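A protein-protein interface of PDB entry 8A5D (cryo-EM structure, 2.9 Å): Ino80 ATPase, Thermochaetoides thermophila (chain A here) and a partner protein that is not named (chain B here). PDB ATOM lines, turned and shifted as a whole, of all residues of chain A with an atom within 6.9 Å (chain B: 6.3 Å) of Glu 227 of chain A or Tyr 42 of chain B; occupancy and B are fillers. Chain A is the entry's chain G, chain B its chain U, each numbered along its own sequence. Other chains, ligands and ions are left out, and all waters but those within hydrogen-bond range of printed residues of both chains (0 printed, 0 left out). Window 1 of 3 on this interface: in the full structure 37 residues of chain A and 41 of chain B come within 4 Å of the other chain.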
ATOM      1  N   ILE A 222     -28.684 -28.442 -13.219  1.00  0.00           N
ATOM      2  CA  ILE A 222     -29.351 -29.453 -14.074  1.00  0.00           C
ATOM      3  C   ILE A 222     -29.925 -28.779 -15.331  1.00  0.00           C
ATOM      4  O   ILE A 222     -29.670 -29.278 -16.428  1.00  0.00           O
ATOM      5  CB  ILE A 222     -30.399 -30.217 -13.268  1.00  0.00           C
ATOM      6  CG1 ILE A 222     -29.712 -31.102 -12.223  1.00  0.00           C
ATOM      7  CG2 ILE A 222     -31.301 -30.985 -14.198  1.00  0.00           C
ATOM      8  CD1 ILE A 222     -30.628 -31.567 -11.131  1.00  0.00           C
ATOM      9  N   LEU A 223     -30.530 -27.620 -15.206  1.00  0.00           N
ATOM     10  CA  LEU A 223     -31.047 -26.877 -16.372  1.00  0.00           C
ATOM     11  C   LEU A 223     -29.874 -26.391 -17.229  1.00  0.00           C
ATOM     12  O   LEU A 223     -29.890 -26.688 -18.429  1.00  0.00           O
ATOM     13  CB  LEU A 223     -31.883 -25.680 -15.902  1.00  0.00           C
ATOM     14  CG  LEU A 223     -33.144 -26.021 -15.110  1.00  0.00           C
ATOM     15  CD1 LEU A 223     -34.051 -24.811 -15.018  1.00  0.00           C
ATOM     16  CD2 LEU A 223     -33.852 -27.194 -15.726  1.00  0.00           C
ATOM     17  N   ALA A 224     -28.891 -25.700 -16.656  1.00  0.00           N
ATOM     18  CA  ALA A 224     -27.775 -25.099 -17.428  1.00  0.00           C
ATOM     19  C   ALA A 224     -26.982 -26.190 -18.151  1.00  0.00           C
ATOM     20  O   ALA A 224     -26.551 -25.922 -19.296  1.00  0.00           O
ATOM     21  CB  ALA A 224     -26.854 -24.240 -16.595  1.00  0.00           C
ATOM     22  N   SER A 225     -26.811 -27.368 -17.559  1.00  0.00           N
ATOM     23  CA  SER A 225     -26.033 -28.446 -18.208  1.00  0.00           C
ATOM     24  C   SER A 225     -26.846 -29.062 -19.345  1.00  0.00           C
ATOM     25  O   SER A 225     -26.186 -29.482 -20.301  1.00  0.00           O
ATOM     26  CB  SER A 225     -25.523 -29.486 -17.247  1.00  0.00           C
ATOM     27  OG  SER A 225     -26.605 -30.063 -16.524  1.00  0.00           O
ATOM     28  N   LYS A 226     -28.179 -29.176 -19.253  1.00  0.00           N
ATOM     29  CA  LYS A 226     -28.999 -29.640 -20.397  1.00  0.00           C
ATOM     30  C   LYS A 226     -28.818 -28.660 -21.575  1.00  0.00           C
ATOM     31  O   LYS A 226     -28.620 -29.130 -22.710  1.00  0.00           O
ATOM     32  CB  LYS A 226     -30.478 -29.743 -20.042  1.00  0.00           C
ATOM     33  CG  LYS A 226     -30.911 -30.985 -19.284  1.00  0.00           C
ATOM     34  CD  LYS A 226     -32.452 -31.098 -19.267  1.00  0.00           C
ATOM     35  CE  LYS A 226     -32.999 -32.337 -18.576  1.00  0.00           C
ATOM     36  NZ  LYS A 226     -34.467 -32.272 -18.352  1.00  0.00           N
ATOM     37  N   GLU A 227     -28.909 -27.353 -21.341  1.00  0.00           N
ATOM     38  CA  GLU A 227     -28.788 -26.330 -22.402  1.00  0.00           C
ATOM     39  C   GLU A 227     -27.430 -26.466 -23.104  1.00  0.00           C
ATOM     40  O   GLU A 227     -27.406 -26.395 -24.349  1.00  0.00           O
ATOM     41  CB  GLU A 227     -28.904 -24.917 -21.841  1.00  0.00           C
ATOM     42  CG  GLU A 227     -30.228 -24.663 -21.201  1.00  0.00           C
ATOM     43  CD  GLU A 227     -31.363 -24.975 -22.142  1.00  0.00           C
ATOM     44  OE1 GLU A 227     -31.498 -24.200 -23.089  1.00  0.00           O
ATOM     45  OE2 GLU A 227     -32.061 -26.009 -21.958  1.00  0.00           O
ATOM     46  N   ALA A 228     -26.345 -26.578 -22.365  1.00  0.00           N
ATOM     47  CA  ALA A 228     -24.991 -26.647 -22.946  1.00  0.00           C
ATOM     48  C   ALA A 228     -24.910 -27.792 -23.981  1.00  0.00           C
ATOM     49  O   ALA A 228     -24.186 -27.608 -24.986  1.00  0.00           O
ATOM     50  CB  ALA A 228     -23.905 -26.738 -21.869  1.00  0.00           C
ATOM     51  N   LYS A 229     -25.574 -28.921 -23.767  1.00  0.00           N
ATOM     52  CA  LYS A 229     -25.481 -30.088 -24.687  1.00  0.00           C
ATOM     53  C   LYS A 229     -26.535 -30.020 -25.831  1.00  0.00           C
ATOM     54  O   LYS A 229     -26.338 -30.676 -26.811  1.00  0.00           O
ATOM     55  CB  LYS A 229     -25.655 -31.378 -23.888  1.00  0.00           C
ATOM     56  CG  LYS A 229     -24.768 -31.565 -22.661  1.00  0.00           C
ATOM     57  CD  LYS A 229     -24.884 -32.927 -21.974  1.00  0.00           C
ATOM     58  CE  LYS A 229     -26.165 -33.146 -21.184  1.00  0.00           C
ATOM     59  NZ  LYS A 229     -26.465 -34.587 -20.915  1.00  0.00           N
ATOM     60  N   ARG A 230     -27.630 -29.277 -25.741  1.00  0.00           N
ATOM     61  CA  ARG A 230     -28.835 -29.524 -26.580  1.00  0.00           C
ATOM     62  C   ARG A 230     -28.560 -29.301 -28.065  1.00  0.00           C
ATOM     63  O   ARG A 230     -29.242 -29.964 -28.871  1.00  0.00           O
ATOM     64  CB  ARG A 230     -30.064 -28.703 -26.166  1.00  0.00           C
ATOM     65  CG  ARG A 230     -31.256 -28.984 -27.072  1.00  0.00           C
ATOM     66  CD  ARG A 230     -32.460 -28.065 -26.988  1.00  0.00           C
ATOM     67  NE  ARG A 230     -32.048 -26.670 -26.854  1.00  0.00           N
ATOM     68  CZ  ARG A 230     -32.185 -25.923 -25.753  1.00  0.00           C
ATOM     69  NH1 ARG A 230     -32.747 -26.409 -24.646  1.00  0.00           N
ATOM     70  NH2 ARG A 230     -31.749 -24.675 -25.770  1.00  0.00           N
ATOM     71  N   TRP A 231     -27.631 -28.427 -28.451  1.00  0.00           N
ATOM     72  CA  TRP A 231     -27.322 -28.154 -29.891  1.00  0.00           C
ATOM     73  C   TRP A 231     -26.974 -29.449 -30.660  1.00  0.00           C
ATOM     74  O   TRP A 231     -27.146 -29.472 -31.868  1.00  0.00           O
ATOM     75  CB  TRP A 231     -26.204 -27.116 -30.014  1.00  0.00           C
ATOM     76  CG  TRP A 231     -24.866 -27.553 -29.514  1.00  0.00           C
ATOM     77  CD1 TRP A 231     -24.369 -27.370 -28.264  1.00  0.00           C
ATOM     78  CD2 TRP A 231     -23.830 -28.238 -30.228  1.00  0.00           C
ATOM     79  NE1 TRP A 231     -23.102 -27.863 -28.142  1.00  0.00           N
ATOM     80  CE2 TRP A 231     -22.734 -28.389 -29.338  1.00  0.00           C
ATOM     81  CE3 TRP A 231     -23.695 -28.715 -31.533  1.00  0.00           C
ATOM     82  CZ2 TRP A 231     -21.523 -28.976 -29.713  1.00  0.00           C
ATOM     83  CZ3 TRP A 231     -22.515 -29.333 -31.886  1.00  0.00           C
ATOM     84  CH2 TRP A 231     -21.447 -29.471 -30.993  1.00  0.00           C
ATOM     85  N   TYR B  38     -40.605 -23.792 -16.701  1.00  0.00           N
ATOM     86  CA  TYR B  38     -39.454 -22.995 -17.206  1.00  0.00           C
ATOM     87  C   TYR B  38     -39.301 -23.157 -18.720  1.00  0.00           C
ATOM     88  O   TYR B  38     -39.725 -24.166 -19.313  1.00  0.00           O
ATOM     89  CB  TYR B  38     -38.149 -23.344 -16.503  1.00  0.00           C
ATOM     90  CG  TYR B  38     -37.336 -24.402 -17.184  1.00  0.00           C
ATOM     91  CD1 TYR B  38     -37.683 -25.735 -17.106  1.00  0.00           C
ATOM     92  CD2 TYR B  38     -36.192 -24.063 -17.878  1.00  0.00           C
ATOM     93  CE1 TYR B  38     -36.931 -26.711 -17.740  1.00  0.00           C
ATOM     94  CE2 TYR B  38     -35.407 -25.030 -18.486  1.00  0.00           C
ATOM     95  CZ  TYR B  38     -35.781 -26.355 -18.429  1.00  0.00           C
ATOM     96  OH  TYR B  38     -34.995 -27.284 -19.050  1.00  0.00           O
ATOM     97  N   THR B  40     -36.200 -21.617 -21.931  1.00  0.00           N
ATOM     98  CA  THR B  40     -34.831 -21.103 -22.201  1.00  0.00           C
ATOM     99  C   THR B  40     -34.793 -20.331 -23.527  1.00  0.00           C
ATOM    100  O   THR B  40     -35.631 -20.576 -24.389  1.00  0.00           O
ATOM    101  CB  THR B  40     -33.835 -22.261 -22.202  1.00  0.00           C
ATOM    102  OG1 THR B  40     -32.562 -21.617 -22.247  1.00  0.00           O
ATOM    103  CG2 THR B  40     -34.085 -23.227 -23.347  1.00  0.00           C
ATOM    104  N   ASP B  41     -33.839 -19.423 -23.665  1.00  0.00           N
ATOM    105  CA  ASP B  41     -33.629 -18.557 -24.845  1.00  0.00           C
ATOM    106  C   ASP B  41     -32.275 -18.888 -25.491  1.00  0.00           C
ATOM    107  O   ASP B  41     -31.806 -18.102 -26.309  1.00  0.00           O
ATOM    108  CB  ASP B  41     -33.694 -17.105 -24.374  1.00  0.00           C
ATOM    109  CG  ASP B  41     -33.764 -16.056 -25.469  1.00  0.00           C
ATOM    110  OD1 ASP B  41     -34.563 -16.266 -26.414  1.00  0.00           O
ATOM    111  OD2 ASP B  41     -33.025 -15.029 -25.370  1.00  0.00           O
ATOM    112  N   TYR B  42     -31.620 -19.990 -25.152  1.00  0.00           N
ATOM    113  CA  TYR B  42     -30.211 -20.206 -25.570  1.00  0.00           C
ATOM    114  C   TYR B  42     -30.201 -20.902 -26.901  1.00  0.00           C
ATOM    115  O   TYR B  42     -30.782 -21.974 -26.957  1.00  0.00           O
ATOM    116  CB  TYR B  42     -29.433 -21.043 -24.577  1.00  0.00           C
ATOM    117  CG  TYR B  42     -27.996 -21.313 -24.932  1.00  0.00           C
ATOM    118  CD1 TYR B  42     -27.026 -20.342 -24.921  1.00  0.00           C
ATOM    119  CD2 TYR B  42     -27.587 -22.597 -25.092  1.00  0.00           C
ATOM    120  CE1 TYR B  42     -25.689 -20.648 -25.130  1.00  0.00           C
ATOM    121  CE2 TYR B  42     -26.270 -22.924 -25.290  1.00  0.00           C
ATOM    122  CZ  TYR B  42     -25.305 -21.957 -25.340  1.00  0.00           C
ATOM    123  OH  TYR B  42     -24.031 -22.407 -25.584  1.00  0.00           O
ATOM    124  N   MET B  43     -29.576 -20.275 -27.899  1.00  0.00           N
ATOM    125  CA  MET B  43     -29.397 -20.779 -29.278  1.00  0.00           C
ATOM    126  C   MET B  43     -30.740 -21.154 -29.896  1.00  0.00           C
ATOM    127  O   MET B  43     -30.827 -22.174 -30.620  1.00  0.00           O
ATOM    128  CB  MET B  43     -28.427 -21.952 -29.220  1.00  0.00           C
ATOM    129  CG  MET B  43     -26.971 -21.482 -28.932  1.00  0.00           C
ATOM    130  SD  MET B  43     -25.853 -22.911 -28.902  1.00  0.00           S
ATOM    131  CE  MET B  43     -25.955 -23.433 -30.616  1.00  0.00           C
ATOM    132  N   LYS B  44     -31.768 -20.358 -29.617  1.00  0.00           N
ATOM    133  CA  LYS B  44     -33.125 -20.615 -30.125  1.00  0.00           C
ATOM    134  C   LYS B  44     -33.315 -19.967 -31.496  1.00  0.00           C
ATOM    135  O   LYS B  44     -34.269 -20.352 -32.190  1.00  0.00           O
ATOM    136  CB  LYS B  44     -34.135 -20.137 -29.084  1.00  0.00           C
ATOM    137  CG  LYS B  44     -34.399 -21.149 -27.984  1.00  0.00           C
ATOM    138  CD  LYS B  44     -35.025 -22.482 -28.358  1.00  0.00           C
ATOM    139  CE  LYS B  44     -35.303 -23.336 -27.117  1.00  0.00           C
ATOM    140  NZ  LYS B  44     -35.919 -24.667 -27.399  1.00  0.00           N
ATOM    141  N   ARG B  45     -32.492 -18.985 -31.856  1.00  0.00           N
ATOM    142  CA  ARG B  45     -32.653 -18.164 -33.095  1.00  0.00           C
ATOM    143  C   ARG B  45     -31.318 -18.081 -33.833  1.00  0.00           C
ATOM    144  O   ARG B  45     -30.301 -18.014 -33.149  1.00  0.00           O
ATOM    145  CB  ARG B  45     -33.135 -16.764 -32.729  1.00  0.00           C
ATOM    146  CG  ARG B  45     -34.506 -16.764 -32.078  1.00  0.00           C
ATOM    147  CD  ARG B  45     -34.934 -15.390 -31.616  1.00  0.00           C
ATOM    148  NE  ARG B  45     -34.163 -14.879 -30.489  1.00  0.00           N
ATOM    149  CZ  ARG B  45     -33.274 -13.883 -30.535  1.00  0.00           C
ATOM    150  NH1 ARG B  45     -32.970 -13.259 -31.667  1.00  0.00           N
ATOM    151  NH2 ARG B  45     -32.683 -13.502 -29.411  1.00  0.00           N
ATOM    152  N   GLN B  48     -28.349 -15.868 -32.894  1.00  0.00           N
ATOM    153  CA  GLN B  48     -27.611 -16.211 -31.663  1.00  0.00           C
ATOM    154  C   GLN B  48     -26.523 -17.217 -31.930  1.00  0.00           C
ATOM    155  O   GLN B  48     -25.739 -17.455 -30.972  1.00  0.00           O
ATOM    156  CB  GLN B  48     -28.543 -16.876 -30.666  1.00  0.00           C
ATOM    157  CG  GLN B  48     -29.521 -15.896 -30.069  1.00  0.00           C
ATOM    158  CD  GLN B  48     -30.518 -16.619 -29.223  1.00  0.00           C
ATOM    159  OE1 GLN B  48     -30.922 -17.733 -29.548  1.00  0.00           O
ATOM    160  NE2 GLN B  48     -30.854 -16.007 -28.103  1.00  0.00           N
ATOM    161  N   ARG B 737     -16.105 -27.084 -32.893  1.00  0.00           N
ATOM    162  CA  ARG B 737     -17.584 -27.014 -32.757  1.00  0.00           C
ATOM    163  C   ARG B 737     -18.243 -26.452 -34.034  1.00  0.00           C
ATOM    164  O   ARG B 737     -19.380 -26.808 -34.331  1.00  0.00           O
ATOM    165  CB  ARG B 737     -17.950 -26.196 -31.513  1.00  0.00           C
ATOM    166  CG  ARG B 737     -19.443 -26.174 -31.217  1.00  0.00           C
ATOM    167  CD  ARG B 737     -19.697 -25.424 -29.941  1.00  0.00           C
ATOM    168  NE  ARG B 737     -21.107 -25.216 -29.767  1.00  0.00           N
ATOM    169  CZ  ARG B 737     -21.646 -24.258 -29.030  1.00  0.00           C
ATOM    170  NH1 ARG B 737     -20.892 -23.406 -28.343  1.00  0.00           N
ATOM    171  NH2 ARG B 737     -22.965 -24.147 -29.003  1.00  0.00           N
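Printed residues of chain B that touch a printed residue of chain A: Tyr 38, Thr 40, Tyr 42, Met 43 and Arg 737.
Among the printed residues, no Asp or Glu carboxylate lies within 4 Å of a Lys or Arg side-chain nitrogen of the other chain.
The side-chain carboxylate (OE1) of Glu 227 of chain A sits close to the side-chain hydroxyl (OG1) of Thr 40 of chain B, 2.9 Å away.
The guanidinium group (NH2) of Arg 230 of chain A lies within hydrogen-bond range of the backbone carbonyl oxygen (O) of Tyr 42 of chain B, 3.1 Å away.
Ala 224 of chain A touches none of the printed residues of chain B.
Of chain B, only Thr 40 and Tyr 42 come within 4 Å of Glu 227 of chain A.
Printed residues of chain B within 4 Å of Trp 231 of chain A: Met 43 (3.7 Å) and Arg 737 (3.6 Å).
Of chain A, only Glu 227 and Arg 230 come within 4 Å of Tyr 42 of chain B.
Of the printed residues of chain A, Met 43 of chain B touches Trp 231 (3.7 Å).
Lys 44 of chain B touches none of the printed residues of chain A.
The nearest residue of chain B that does not touch Glu 227 of chain A is Tyr 38 of chain B (4.3 Å).
The nearest residue of chain A that does not touch Tyr 42 of chain B is Ala 228 of chain A (4.6 Å).
The nearest printed residue of chain A that does not touch Met 43 of chain B is Arg 230 of chain A (5.3 Å).
CZ of Tyr 38 of chain B touches CD2 of Leu 223 of chain A, 3.4 Å away.
O of Glu 227 of chain A touches CE2 of Tyr 42 of chain B, 3.8 Å away.
Arg 230 of chain A touches Thr 40 of chain B (NH2 to CG2, 3.7 Å).
CB of Trp 231 of chain A touches CE of Met 43 of chain B, 3.7 Å away.
Arg 737 of chain B touches Trp 231 of chain A.
OE1 of Glu 227 of chain A lies within salt-bridge range of NH2 of Arg 230 of chain A (2.7 Å).
O of Ala 228 of chain A sits close to NE1 of Trp 231 of chain A, 3.3 Å away.
OG1 of Thr 40 of chain B sits at hydrogen-bond distance from N of Tyr 42 of chain B (3.5 Å).
The side-chain amide oxygen (OE1) of Gln 48 of chain B lies within hydrogen-bond range of the backbone NH (N) of Met 43 of chain B (3.3 Å).
SD of Met 43 of chain B lies within hydrogen-bond range of NH2 of Arg 737 of chain B.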
